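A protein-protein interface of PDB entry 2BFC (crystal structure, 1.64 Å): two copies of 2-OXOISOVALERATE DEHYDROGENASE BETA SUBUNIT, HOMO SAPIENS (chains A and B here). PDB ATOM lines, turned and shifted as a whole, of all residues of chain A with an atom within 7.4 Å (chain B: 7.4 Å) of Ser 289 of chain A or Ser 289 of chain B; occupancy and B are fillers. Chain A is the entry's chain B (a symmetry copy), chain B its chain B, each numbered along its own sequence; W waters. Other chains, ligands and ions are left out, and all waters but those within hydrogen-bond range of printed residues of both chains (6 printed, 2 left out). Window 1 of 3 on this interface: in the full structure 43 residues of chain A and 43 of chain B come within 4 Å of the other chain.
The backbone NH of Gly 285 of chain B sits at hydrogen-bond distance from the side-chain carboxylate of Glu 290 of chain A (2.8 Å).
OG of Ser 289 of chain B lies within hydrogen-bond range of OG of Ser 289 of chain A (3.3 Å).
The backbone NH (N) of Gly 285 of chain A is in hydrogen-bond range of the side-chain carboxylate (OE1) of Glu 290 of chain B.
NH2 of Arg 309 of chain A is in salt-bridge range of OE2 of Glu 290 of chain B (3.0 Å).
OG of Ser 293 of chain B sits close to NH2 of Arg 309 of chain A (3.4 Å).
The side-chain hydroxyl of Thr 294 of chain B lies within hydrogen-bond range of the guanidinium group of Arg 309 of chain A.
The side-chain carboxylate (OE2) of Glu 297 of chain B is in salt-bridge range of the guanidinium group (NE) of Arg 309 of chain A (2.8 Å).
The side-chain carboxylate of Glu 290 of chain A lies within salt-bridge range of the guanidinium group of Arg 309 of chain B, at 3.0 Å.
OG of Ser 293 of chain A sits close to NH2 of Arg 309 of chain B, 3.4 Å away.
The guanidinium group (NH2) of Arg 309 of chain B sits at hydrogen-bond distance from the side-chain hydroxyl (OG1) of Thr 294 of chain A, 3.3 Å away.
The guanidinium group of Arg 309 of chain B is in salt-bridge range of the side-chain carboxylate of Glu 297 of chain A (2.8 Å).
The backbone carbonyl oxygen of Gly 286 of chain B is in hydrogen-bond range of the side-chain hydroxyl of Ser 289 of chain B (2.7 Å).
The backbone carbonyl oxygen (O) of Glu 290 of chain B lies within hydrogen-bond range of the side-chain hydroxyl (OG1) of Thr 294 of chain B, at 2.9 Å.
Among the printed residues, merely in contact across the chains: Leu 283 of chain A with Glu 290 of chain B (3.6 Å), Thr 284 of chain A with Glu 290 of chain B (3.6 Å), Ser 289 of chain A with Glu 290 of chain B (3.6 Å), Ser 289 of chain A with Ser 293 of chain B (3.5 Å), Glu 290 of chain A with Leu 283 of chain B (3.6 Å), Glu 290 of chain A with Thr 284 of chain B (3.6 Å), Glu 290 of chain A with Ser 289 of chain B (3.6 Å), Ser 292 of chain A with Ser 293 of chain B (3.6 Å), Ser 293 of chain A with Ser 289 of chain B (3.5 Å) and Ser 293 of chain A with Ser 292 of chain B (3.6 Å).
Printed residues of chain B within 4 Å of Ser 289 of chain A: Ser 289, Glu 290 and Ser 293.
No residue of chain B comes within 4 Å of Ala 288 of chain A.
Of the printed residues of chain A, Glu 290 of chain B touches Leu 283, Thr 284, Gly 285, Ser 289 and Arg 309.
Of the 20 printed residues of chain B, 10 touch a printed residue of chain A.
Among the printed residues, 21 pairs touch across the chains.
Ser 289 of chain A touches its own counterpart, Ser 289 of chain B.
Ser 292 of chain A touches Ser 293 of chain B, and with the chains exchanged Ser 293 of chain A touches Ser 292 of chain B.
Water W5 lies within hydrogen-bond range of the side-chain hydroxyl of Ser 292 of chain A (2.6 Å) and the side-chain carboxylate of Glu 297 of chain B (2.7 Å).
Water W2 bridges O of Ala 152 of chain A (2.7 Å) and O of Gly 285 of chain B (3.1 Å).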
ATOM      1  N   ALA A 152     -28.129  10.349 -25.192  1.00  0.00           N
ATOM      2  CA  ALA A 152     -28.549   9.370 -24.175  1.00  0.00           C
ATOM      3  C   ALA A 152     -30.037   9.248 -24.099  1.00  0.00           C
ATOM      4  O   ALA A 152     -30.549   8.230 -23.643  1.00  0.00           O
ATOM      5  CB  ALA A 152     -28.009   9.815 -22.790  1.00  0.00           C
ATOM      6  N   TRP A 227     -16.678  10.603 -28.154  1.00  0.00           N
ATOM      7  CA  TRP A 227     -17.270  10.656 -29.496  1.00  0.00           C
ATOM      8  C   TRP A 227     -17.441  12.092 -29.861  1.00  0.00           C
ATOM      9  O   TRP A 227     -17.390  12.958 -29.003  1.00  0.00           O
ATOM     10  CB  TRP A 227     -18.651   9.918 -29.606  1.00  0.00           C
ATOM     11  CG  TRP A 227     -19.617  10.160 -28.446  1.00  0.00           C
ATOM     12  CD1 TRP A 227     -20.585  11.125 -28.359  1.00  0.00           C
ATOM     13  CD2 TRP A 227     -19.661   9.436 -27.202  1.00  0.00           C
ATOM     14  NE1 TRP A 227     -21.266  11.025 -27.169  1.00  0.00           N
ATOM     15  CE2 TRP A 227     -20.705  10.000 -26.423  1.00  0.00           C
ATOM     16  CE3 TRP A 227     -18.941   8.335 -26.686  1.00  0.00           C
ATOM     17  CZ2 TRP A 227     -21.063   9.492 -25.123  1.00  0.00           C
ATOM     18  CZ3 TRP A 227     -19.270   7.850 -25.380  1.00  0.00           C
ATOM     19  CH2 TRP A 227     -20.328   8.423 -24.628  1.00  0.00           C
ATOM     20  N   ILE A 277     -14.235   7.710 -19.459  1.00  0.00           N
ATOM     21  CA  ILE A 277     -15.227   8.006 -20.527  1.00  0.00           C
ATOM     22  C   ILE A 277     -15.586   9.473 -20.379  1.00  0.00           C
ATOM     23  O   ILE A 277     -15.787   9.918 -19.262  1.00  0.00           O
ATOM     24  CB  ILE A 277     -16.566   7.155 -20.419  1.00  0.00           C
ATOM     25  CG1 ILE A 277     -16.290   5.645 -20.254  1.00  0.00           C
ATOM     26  CG2 ILE A 277     -17.477   7.424 -21.642  1.00  0.00           C
ATOM     27  CD1 ILE A 277     -17.315   4.931 -19.376  1.00  0.00           C
ATOM     28  N   HIS A 279     -17.952  12.846 -22.076  1.00  0.00           N
ATOM     29  CA  HIS A 279     -18.914  13.404 -23.019  1.00  0.00           C
ATOM     30  C   HIS A 279     -19.436  14.747 -22.536  1.00  0.00           C
ATOM     31  O   HIS A 279     -19.536  14.971 -21.349  1.00  0.00           O
ATOM     32  CB  HIS A 279     -20.110  12.451 -23.308  1.00  0.00           C
ATOM     33  CG  HIS A 279     -20.958  12.050 -22.122  1.00  0.00           C
ATOM     34  ND1 HIS A 279     -21.172  10.719 -21.788  1.00  0.00           N
ATOM     35  CD2 HIS A 279     -21.739  12.778 -21.287  1.00  0.00           C
ATOM     36  CE1 HIS A 279     -22.037  10.646 -20.769  1.00  0.00           C
ATOM     37  NE2 HIS A 279     -22.406  11.888 -20.470  1.00  0.00           N
ATOM     38  N   LEU A 283     -23.749  14.328 -16.802  1.00  0.00           N
ATOM     39  CA  LEU A 283     -23.326  13.038 -16.161  1.00  0.00           C
ATOM     40  C   LEU A 283     -24.540  12.147 -15.956  1.00  0.00           C
ATOM     41  O   LEU A 283     -24.539  11.004 -16.417  1.00  0.00           O
ATOM     42  CB  LEU A 283     -22.731  13.372 -14.787  1.00  0.00           C
ATOM     43  CG  LEU A 283     -22.367  12.128 -13.982  1.00  0.00           C
ATOM     44  CD1 LEU A 283     -21.142  11.480 -14.632  1.00  0.00           C
ATOM     45  CD2 LEU A 283     -22.111  12.602 -12.579  1.00  0.00           C
ATOM     46  N   THR A 284     -25.596  12.642 -15.298  1.00  0.00           N
ATOM     47  CA  THR A 284     -26.643  11.671 -14.801  1.00  0.00           C
ATOM     48  C   THR A 284     -27.468  11.155 -15.975  1.00  0.00           C
ATOM     49  O   THR A 284     -28.037  11.941 -16.742  1.00  0.00           O
ATOM     50  CB  THR A 284     -27.476  12.292 -13.713  1.00  0.00           C
ATOM     51  OG1 THR A 284     -26.621  12.570 -12.600  1.00  0.00           O
ATOM     52  CG2 THR A 284     -28.526  11.297 -13.145  1.00  0.00           C
ATOM     53  N   GLY A 285     -27.502   9.823 -16.130  1.00  0.00           N
ATOM     54  CA  GLY A 285     -28.319   9.268 -17.251  1.00  0.00           C
ATOM     55  C   GLY A 285     -27.585   9.410 -18.560  1.00  0.00           C
ATOM     56  O   GLY A 285     -28.083   8.946 -19.590  1.00  0.00           O
ATOM     57  N   GLY A 286     -26.363   9.955 -18.546  1.00  0.00           N
ATOM     58  CA  GLY A 286     -25.614  10.118 -19.824  1.00  0.00           C
ATOM     59  C   GLY A 286     -25.065   8.780 -20.318  1.00  0.00           C
ATOM     60  O   GLY A 286     -25.133   7.775 -19.587  1.00  0.00           O
ATOM     61  N   PHE A 287     -24.609   8.723 -21.576  1.00  0.00           N
ATOM     62  CA  PHE A 287     -24.290   7.382 -22.121  1.00  0.00           C
ATOM     63  C   PHE A 287     -23.048   6.792 -21.479  1.00  0.00           C
ATOM     64  O   PHE A 287     -22.854   5.590 -21.510  1.00  0.00           O
ATOM     65  CB  PHE A 287     -24.220   7.400 -23.678  1.00  0.00           C
ATOM     66  CG  PHE A 287     -24.250   6.004 -24.266  1.00  0.00           C
ATOM     67  CD1 PHE A 287     -25.375   5.237 -24.119  1.00  0.00           C
ATOM     68  CD2 PHE A 287     -23.133   5.453 -24.894  1.00  0.00           C
ATOM     69  CE1 PHE A 287     -25.475   3.930 -24.635  1.00  0.00           C
ATOM     70  CE2 PHE A 287     -23.172   4.126 -25.360  1.00  0.00           C
ATOM     71  CZ  PHE A 287     -24.309   3.356 -25.233  1.00  0.00           C
ATOM     72  N   ALA A 288     -22.218   7.617 -20.817  1.00  0.00           N
ATOM     73  CA  ALA A 288     -21.081   7.039 -20.106  1.00  0.00           C
ATOM     74  C   ALA A 288     -21.501   6.057 -19.034  1.00  0.00           C
ATOM     75  O   ALA A 288     -20.746   5.130 -18.706  1.00  0.00           O
ATOM     76  CB  ALA A 288     -20.199   8.149 -19.458  1.00  0.00           C
ATOM     77  N   SER A 289     -22.685   6.223 -18.467  1.00  0.00           N
ATOM     78  CA  SER A 289     -23.169   5.263 -17.436  1.00  0.00           C
ATOM     79  C   SER A 289     -23.356   3.871 -18.022  1.00  0.00           C
ATOM     80  O   SER A 289     -23.034   2.877 -17.366  1.00  0.00           O
ATOM     81  CB  SER A 289     -24.492   5.713 -16.805  1.00  0.00           C
ATOM     82  OG  SER A 289     -25.489   5.853 -17.796  1.00  0.00           O
ATOM     83  N   GLU A 290     -23.882   3.791 -19.247  1.00  0.00           N
ATOM     84  CA  GLU A 290     -24.100   2.459 -19.911  1.00  0.00           C
ATOM     85  C   GLU A 290     -22.764   1.813 -20.208  1.00  0.00           C
ATOM     86  O   GLU A 290     -22.546   0.596 -19.954  1.00  0.00           O
ATOM     87  CB  GLU A 290     -24.960   2.615 -21.194  1.00  0.00           C
ATOM     88  CG  GLU A 290     -25.235   1.235 -21.880  1.00  0.00           C
ATOM     89  CD  GLU A 290     -25.974   0.310 -20.970  1.00  0.00           C
ATOM     90  OE1 GLU A 290     -26.859   0.796 -20.246  1.00  0.00           O
ATOM     91  OE2 GLU A 290     -25.646  -0.886 -20.915  1.00  0.00           O
ATOM     92  N   ILE A 291     -21.814   2.600 -20.680  1.00  0.00           N
ATOM     93  CA  ILE A 291     -20.494   2.007 -21.031  1.00  0.00           C
ATOM     94  C   ILE A 291     -19.813   1.540 -19.752  1.00  0.00           C
ATOM     95  O   ILE A 291     -19.216   0.444 -19.712  1.00  0.00           O
ATOM     96  CB  ILE A 291     -19.648   3.049 -21.779  1.00  0.00           C
ATOM     97  CG1 ILE A 291     -20.327   3.377 -23.109  1.00  0.00           C
ATOM     98  CG2 ILE A 291     -18.223   2.508 -22.017  1.00  0.00           C
ATOM     99  CD1 ILE A 291     -19.695   4.618 -23.802  1.00  0.00           C
ATOM    100  N   SER A 292     -19.876   2.391 -18.734  1.00  0.00           N
ATOM    101  CA  SER A 292     -19.220   2.078 -17.458  1.00  0.00           C
ATOM    102  C   SER A 292     -19.791   0.819 -16.853  1.00  0.00           C
ATOM    103  O   SER A 292     -19.057  -0.112 -16.494  1.00  0.00           O
ATOM    104  CB  SER A 292     -19.411   3.266 -16.490  1.00  0.00           C
ATOM    105  OG  SER A 292     -18.797   2.896 -15.238  1.00  0.00           O
ATOM    106  N   SER A 293     -21.114   0.761 -16.744  1.00  0.00           N
ATOM    107  CA  SER A 293     -21.742  -0.411 -16.122  1.00  0.00           C
ATOM    108  C   SER A 293     -21.477  -1.700 -16.911  1.00  0.00           C
ATOM    109  O   SER A 293     -21.374  -2.792 -16.310  1.00  0.00           O
ATOM    110  CB  SER A 293     -23.254  -0.185 -15.950  1.00  0.00           C
ATOM    111  OG  SER A 293     -23.837   0.170 -17.179  1.00  0.00           O
ATOM    112  N   THR A 294     -21.388  -1.598 -18.238  1.00  0.00           N
ATOM    113  CA  THR A 294     -21.114  -2.758 -19.070  1.00  0.00           C
ATOM    114  C   THR A 294     -19.665  -3.215 -18.940  1.00  0.00           C
ATOM    115  O   THR A 294     -19.351  -4.419 -18.862  1.00  0.00           O
ATOM    116  CB  THR A 294     -21.456  -2.432 -20.537  1.00  0.00           C
ATOM    117  OG1 THR A 294     -22.893  -2.186 -20.625  1.00  0.00           O
ATOM    118  CG2 THR A 294     -21.194  -3.632 -21.450  1.00  0.00           C
ATOM    119  N   VAL A 295     -18.757  -2.254 -18.995  1.00  0.00           N
ATOM    120  CA  VAL A 295     -17.339  -2.626 -18.868  1.00  0.00           C
ATOM    121  C   VAL A 295     -17.091  -3.219 -17.512  1.00  0.00           C
ATOM    122  O   VAL A 295     -16.330  -4.155 -17.361  1.00  0.00           O
ATOM    123  CB  VAL A 295     -16.442  -1.404 -19.076  1.00  0.00           C
ATOM    124  CG1 VAL A 295     -14.984  -1.727 -18.670  1.00  0.00           C
ATOM    125  CG2 VAL A 295     -16.512  -0.967 -20.541  1.00  0.00           C
ATOM    126  N   GLU A 297     -19.162  -5.000 -15.755  1.00  0.00           N
ATOM    127  CA  GLU A 297     -19.656  -6.384 -15.773  1.00  0.00           C
ATOM    128  C   GLU A 297     -18.680  -7.361 -16.519  1.00  0.00           C
ATOM    129  O   GLU A 297     -18.453  -8.507 -16.043  1.00  0.00           O
ATOM    130  CB  GLU A 297     -21.044  -6.422 -16.441  1.00  0.00           C
ATOM    131  CG  GLU A 297     -22.173  -5.798 -15.624  1.00  0.00           C
ATOM    132  CD  GLU A 297     -23.329  -5.210 -16.479  1.00  0.00           C
ATOM    133  OE1 GLU A 297     -23.312  -5.243 -17.730  1.00  0.00           O
ATOM    134  OE2 GLU A 297     -24.253  -4.630 -15.905  1.00  0.00           O
ATOM    135  N   ARG A 309     -16.014   8.906 -15.151  1.00  0.00           N
ATOM    136  CA  ARG A 309     -16.845   9.590 -16.140  1.00  0.00           C
ATOM    137  C   ARG A 309     -16.599  11.067 -15.999  1.00  0.00           C
ATOM    138  O   ARG A 309     -16.734  11.586 -14.898  1.00  0.00           O
ATOM    139  CB  ARG A 309     -18.325   9.320 -15.907  1.00  0.00           C
ATOM    140  CG  ARG A 309     -18.689   7.865 -16.060  1.00  0.00           C
ATOM    141  CD  ARG A 309     -20.164   7.638 -15.821  1.00  0.00           C
ATOM    142  NE  ARG A 309     -20.552   7.756 -14.432  1.00  0.00           N
ATOM    143  CZ  ARG A 309     -21.804   8.025 -14.095  1.00  0.00           C
ATOM    144  NH1 ARG A 309     -22.694   8.269 -15.031  1.00  0.00           N
ATOM    145  NH2 ARG A 309     -22.134   8.098 -12.843  1.00  0.00           N
ATOM    146  N   CYS A 311     -17.928  14.428 -17.447  1.00  0.00           N
ATOM    147  CA  CYS A 311     -19.046  14.777 -18.263  1.00  0.00           C
ATOM    148  C   CYS A 311     -19.449  16.221 -17.977  1.00  0.00           C
ATOM    149  O   CYS A 311     -18.917  16.861 -17.085  1.00  0.00           O
ATOM    150  CB  CYS A 311     -20.234  13.865 -18.001  1.00  0.00           C
ATOM    151  SG  CYS A 311     -19.848  12.120 -18.217  1.00  0.00           S
ATOM    152  N   ALA B 152     -36.089   6.284 -17.416  1.00  0.00           N
ATOM    153  CA  ALA B 152     -34.701   6.621 -17.779  1.00  0.00           C
ATOM    154  C   ALA B 152     -34.641   7.691 -18.821  1.00  0.00           C
ATOM    155  O   ALA B 152     -33.632   8.378 -18.940  1.00  0.00           O
ATOM    156  CB  ALA B 152     -33.997   5.349 -18.323  1.00  0.00           C
ATOM    157  N   TRP B 227     -37.766  -0.462  -7.844  1.00  0.00           N
ATOM    158  CA  TRP B 227     -38.790   0.558  -7.595  1.00  0.00           C
ATOM    159  C   TRP B 227     -40.064   0.082  -8.207  1.00  0.00           C
ATOM    160  O   TRP B 227     -40.056  -0.823  -9.025  1.00  0.00           O
ATOM    161  CB  TRP B 227     -38.426   1.972  -8.172  1.00  0.00           C
ATOM    162  CG  TRP B 227     -37.820   1.969  -9.576  1.00  0.00           C
ATOM    163  CD1 TRP B 227     -38.485   2.089 -10.768  1.00  0.00           C
ATOM    164  CD2 TRP B 227     -36.429   1.799  -9.909  1.00  0.00           C
ATOM    165  NE1 TRP B 227     -37.604   2.056 -11.822  1.00  0.00           N
ATOM    166  CE2 TRP B 227     -36.325   1.858 -11.324  1.00  0.00           C
ATOM    167  CE3 TRP B 227     -35.253   1.640  -9.143  1.00  0.00           C
ATOM    168  CZ2 TRP B 227     -35.062   1.766 -12.012  1.00  0.00           C
ATOM    169  CZ3 TRP B 227     -34.001   1.512  -9.824  1.00  0.00           C
ATOM    170  CH2 TRP B 227     -33.923   1.590 -11.239  1.00  0.00           C
ATOM    171  N   ILE B 277     -29.416  -4.738  -9.239  1.00  0.00           N
ATOM    172  CA  ILE B 277     -30.436  -3.697  -9.532  1.00  0.00           C
ATOM    173  C   ILE B 277     -31.377  -4.301 -10.559  1.00  0.00           C
ATOM    174  O   ILE B 277     -30.904  -4.927 -11.491  1.00  0.00           O
ATOM    175  CB  ILE B 277     -29.836  -2.356 -10.139  1.00  0.00           C
ATOM    176  CG1 ILE B 277     -28.647  -1.819  -9.314  1.00  0.00           C
ATOM    177  CG2 ILE B 277     -30.944  -1.284 -10.282  1.00  0.00           C
ATOM    178  CD1 ILE B 277     -27.577  -1.135 -10.161  1.00  0.00           C
ATOM    179  N   HIS B 279     -35.072  -3.648 -12.961  1.00  0.00           N
ATOM    180  CA  HIS B 279     -36.186  -2.827 -13.422  1.00  0.00           C
ATOM    181  C   HIS B 279     -36.809  -3.409 -14.680  1.00  0.00           C
ATOM    182  O   HIS B 279     -36.126  -4.021 -15.472  1.00  0.00           O
ATOM    183  CB  HIS B 279     -35.788  -1.343 -13.674  1.00  0.00           C
ATOM    184  CG  HIS B 279     -34.708  -1.097 -14.702  1.00  0.00           C
ATOM    185  ND1 HIS B 279     -33.551  -0.393 -14.398  1.00  0.00           N
ATOM    186  CD2 HIS B 279     -34.664  -1.335 -16.036  1.00  0.00           C
ATOM    187  CE1 HIS B 279     -32.820  -0.230 -15.508  1.00  0.00           C
ATOM    188  NE2 HIS B 279     -33.495  -0.779 -16.514  1.00  0.00           N
ATOM    189  N   LEU B 283     -32.661  -2.881 -20.525  1.00  0.00           N
ATOM    190  CA  LEU B 283     -31.279  -2.790 -19.945  1.00  0.00           C
ATOM    191  C   LEU B 283     -30.575  -1.560 -20.495  1.00  0.00           C
ATOM    192  O   LEU B 283     -30.104  -0.731 -19.715  1.00  0.00           O
ATOM    193  CB  LEU B 283     -30.502  -4.035 -20.392  1.00  0.00           C
ATOM    194  CG  LEU B 283     -29.039  -4.005 -19.961  1.00  0.00           C
ATOM    195  CD1 LEU B 283     -28.983  -4.208 -18.444  1.00  0.00           C
ATOM    196  CD2 LEU B 283     -28.357  -5.101 -20.730  1.00  0.00           C
ATOM    197  N   THR B 284     -30.508  -1.398 -21.823  1.00  0.00           N
ATOM    198  CA  THR B 284     -29.531  -0.381 -22.367  1.00  0.00           C
ATOM    199  C   THR B 284     -30.050   1.028 -22.102  1.00  0.00           C
ATOM    200  O   THR B 284     -31.178   1.369 -22.482  1.00  0.00           O
ATOM    201  CB  THR B 284     -29.235  -0.645 -23.818  1.00  0.00           C
ATOM    202  OG1 THR B 284     -28.591  -1.919 -23.917  1.00  0.00           O
ATOM    203  CG2 THR B 284     -28.190   0.353 -24.389  1.00  0.00           C
ATOM    204  N   GLY B 285     -29.230   1.838 -21.415  1.00  0.00           N
ATOM    205  CA  GLY B 285     -29.684   3.237 -21.154  1.00  0.00           C
ATOM    206  C   GLY B 285     -30.677   3.268 -20.021  1.00  0.00           C
ATOM    207  O   GLY B 285     -31.113   4.351 -19.622  1.00  0.00           O
ATOM    208  N   GLY B 286     -30.984   2.114 -19.415  1.00  0.00           N
ATOM    209  CA  GLY B 286     -31.968   2.108 -18.296  1.00  0.00           C
ATOM    210  C   GLY B 286     -31.354   2.673 -17.016  1.00  0.00           C
ATOM    211  O   GLY B 286     -30.134   2.913 -16.968  1.00  0.00           O
ATOM    212  N   PHE B 287     -32.186   2.980 -16.013  1.00  0.00           N
ATOM    213  CA  PHE B 287     -31.620   3.733 -14.868  1.00  0.00           C
ATOM    214  C   PHE B 287     -30.683   2.875 -14.037  1.00  0.00           C
ATOM    215  O   PHE B 287     -29.854   3.398 -13.314  1.00  0.00           O
ATOM    216  CB  PHE B 287     -32.738   4.410 -14.020  1.00  0.00           C
ATOM    217  CG  PHE B 287     -32.182   5.457 -13.076  1.00  0.00           C
ATOM    218  CD1 PHE B 287     -31.601   6.585 -13.591  1.00  0.00           C
ATOM    219  CD2 PHE B 287     -32.184   5.268 -11.694  1.00  0.00           C
ATOM    220  CE1 PHE B 287     -31.059   7.600 -12.776  1.00  0.00           C
ATOM    221  CE2 PHE B 287     -31.590   6.226 -10.852  1.00  0.00           C
ATOM    222  CZ  PHE B 287     -31.020   7.374 -11.364  1.00  0.00           C
ATOM    223  N   ALA B 288     -30.744   1.540 -14.178  1.00  0.00           N
ATOM    224  CA  ALA B 288     -29.773   0.717 -13.464  1.00  0.00           C
ATOM    225  C   ALA B 288     -28.344   1.029 -13.853  1.00  0.00           C
ATOM    226  O   ALA B 288     -27.422   0.842 -13.047  1.00  0.00           O
ATOM    227  CB  ALA B 288     -30.041  -0.801 -13.696  1.00  0.00           C
ATOM    228  N   SER B 289     -28.120   1.501 -15.070  1.00  0.00           N
ATOM    229  CA  SER B 289     -26.739   1.865 -15.494  1.00  0.00           C
ATOM    230  C   SER B 289     -26.193   3.019 -14.664  1.00  0.00           C
ATOM    231  O   SER B 289     -25.013   3.015 -14.305  1.00  0.00           O
ATOM    232  CB  SER B 289     -26.675   2.252 -16.976  1.00  0.00           C
ATOM    233  OG  SER B 289     -27.532   3.343 -17.240  1.00  0.00           O
ATOM    234  N   GLU B 290     -27.038   4.009 -14.367  1.00  0.00           N
ATOM    235  CA  GLU B 290     -26.591   5.189 -13.548  1.00  0.00           C
ATOM    236  C   GLU B 290     -26.279   4.741 -12.137  1.00  0.00           C
ATOM    237  O   GLU B 290     -25.235   5.119 -11.537  1.00  0.00           O
ATOM    238  CB  GLU B 290     -27.659   6.314 -13.570  1.00  0.00           C
ATOM    239  CG  GLU B 290     -27.198   7.570 -12.757  1.00  0.00           C
ATOM    240  CD  GLU B 290     -25.941   8.152 -13.318  1.00  0.00           C
ATOM    241  OE1 GLU B 290     -25.812   8.168 -14.554  1.00  0.00           O
ATOM    242  OE2 GLU B 290     -25.047   8.536 -12.547  1.00  0.00           O
ATOM    243  N   ILE B 291     -27.115   3.878 -11.587  1.00  0.00           N
ATOM    244  CA  ILE B 291     -26.880   3.438 -10.185  1.00  0.00           C
ATOM    245  C   ILE B 291     -25.605   2.606 -10.142  1.00  0.00           C
ATOM    246  O   ILE B 291     -24.778   2.755  -9.218  1.00  0.00           O
ATOM    247  CB  ILE B 291     -28.096   2.641  -9.688  1.00  0.00           C
ATOM    248  CG1 ILE B 291     -29.309   3.572  -9.637  1.00  0.00           C
ATOM    249  CG2 ILE B 291     -27.811   2.047  -8.293  1.00  0.00           C
ATOM    250  CD1 ILE B 291     -30.638   2.792  -9.416  1.00  0.00           C
ATOM    251  N   SER B 292     -25.479   1.713 -11.116  1.00  0.00           N
ATOM    252  CA  SER B 292     -24.316   0.818 -11.162  1.00  0.00           C
ATOM    253  C   SER B 292     -23.034   1.605 -11.286  1.00  0.00           C
ATOM    254  O   SER B 292     -22.088   1.420 -10.509  1.00  0.00           O
ATOM    255  CB  SER B 292     -24.468  -0.143 -12.362  1.00  0.00           C
ATOM    256  OG  SER B 292     -23.283  -0.967 -12.398  1.00  0.00           O
ATOM    257  N   SER B 293     -22.987   2.510 -12.259  1.00  0.00           N
ATOM    258  CA  SER B 293     -21.757   3.282 -12.473  1.00  0.00           C
ATOM    259  C   SER B 293     -21.403   4.160 -11.265  1.00  0.00           C
ATOM    260  O   SER B 293     -20.205   4.388 -10.987  1.00  0.00           O
ATOM    261  CB  SER B 293     -21.873   4.138 -13.746  1.00  0.00           C
ATOM    262  OG  SER B 293     -23.028   4.937 -13.693  1.00  0.00           O
ATOM    263  N   THR B 294     -22.415   4.672 -10.563  1.00  0.00           N
ATOM    264  CA  THR B 294     -22.181   5.494  -9.388  1.00  0.00           C
ATOM    265  C   THR B 294     -21.692   4.664  -8.206  1.00  0.00           C
ATOM    266  O   THR B 294     -20.777   5.051  -7.453  1.00  0.00           O
ATOM    267  CB  THR B 294     -23.473   6.253  -9.025  1.00  0.00           C
ATOM    268  OG1 THR B 294     -23.785   7.168 -10.120  1.00  0.00           O
ATOM    269  CG2 THR B 294     -23.270   7.144  -7.798  1.00  0.00           C
ATOM    270  N   VAL B 295     -22.355   3.540  -7.986  1.00  0.00           N
ATOM    271  CA  VAL B 295     -21.929   2.686  -6.865  1.00  0.00           C
ATOM    272  C   VAL B 295     -20.535   2.189  -7.111  1.00  0.00           C
ATOM    273  O   VAL B 295     -19.731   2.086  -6.204  1.00  0.00           O
ATOM    274  CB  VAL B 295     -22.884   1.503  -6.696  1.00  0.00           C
ATOM    275  CG1 VAL B 295     -22.290   0.464  -5.716  1.00  0.00           C
ATOM    276  CG2 VAL B 295     -24.238   2.011  -6.194  1.00  0.00           C
ATOM    277  N   GLU B 297     -18.147   3.760  -8.653  1.00  0.00           N
ATOM    278  CA  GLU B 297     -17.218   4.854  -8.341  1.00  0.00           C
ATOM    279  C   GLU B 297     -17.014   5.048  -6.797  1.00  0.00           C
ATOM    280  O   GLU B 297     -15.861   5.277  -6.339  1.00  0.00           O
ATOM    281  CB  GLU B 297     -17.741   6.162  -8.966  1.00  0.00           C
ATOM    282  CG  GLU B 297     -17.656   6.232 -10.489  1.00  0.00           C
ATOM    283  CD  GLU B 297     -18.738   7.130 -11.148  1.00  0.00           C
ATOM    284  OE1 GLU B 297     -19.606   7.728 -10.472  1.00  0.00           O
ATOM    285  OE2 GLU B 297     -18.784   7.195 -12.377  1.00  0.00           O
ATOM    286  N   ARG B 309     -27.279  -6.172 -13.304  1.00  0.00           N
ATOM    287  CA  ARG B 309     -28.506  -5.489 -13.708  1.00  0.00           C
ATOM    288  C   ARG B 309     -29.425  -6.518 -14.304  1.00  0.00           C
ATOM    289  O   ARG B 309     -29.012  -7.223 -15.217  1.00  0.00           O
ATOM    290  CB  ARG B 309     -28.230  -4.419 -14.755  1.00  0.00           C
ATOM    291  CG  ARG B 309     -27.341  -3.313 -14.247  1.00  0.00           C
ATOM    292  CD  ARG B 309     -27.090  -2.273 -15.313  1.00  0.00           C
ATOM    293  NE  ARG B 309     -26.204  -2.722 -16.366  1.00  0.00           N
ATOM    294  CZ  ARG B 309     -26.218  -2.149 -17.560  1.00  0.00           C
ATOM    295  NH1 ARG B 309     -27.104  -1.214 -17.825  1.00  0.00           N
ATOM    296  NH2 ARG B 309     -25.395  -2.549 -18.478  1.00  0.00           N
ATOM    297  N   CYS B 311     -32.880  -6.702 -16.091  1.00  0.00           N
ATOM    298  CA  CYS B 311     -33.765  -5.721 -16.630  1.00  0.00           C
ATOM    299  C   CYS B 311     -34.593  -6.347 -17.749  1.00  0.00           C
ATOM    300  O   CYS B 311     -34.377  -7.483 -18.135  1.00  0.00           O
ATOM    301  CB  CYS B 311     -33.004  -4.525 -17.181  1.00  0.00           C
ATOM    302  SG  CYS B 311     -31.917  -3.759 -15.968  1.00  0.00           S
HETATM  303  O   HOH W   1     -25.516  -7.397 -15.192  1.00  0.00           O
HETATM  304  O   HOH W   2     -30.155   6.457 -21.663  1.00  0.00           O
HETATM  305  O   HOH W   3     -30.959   8.115 -18.846  1.00  0.00           O
HETATM  306  O   HOH W   4     -16.408   9.221 -12.338  1.00  0.00           O
HETATM  307  O   HOH W   5     -18.070   4.938 -13.724  1.00  0.00           O
HETATM  308  O   HOH W   6     -23.595  -3.284 -13.631  1.00  0.00           O
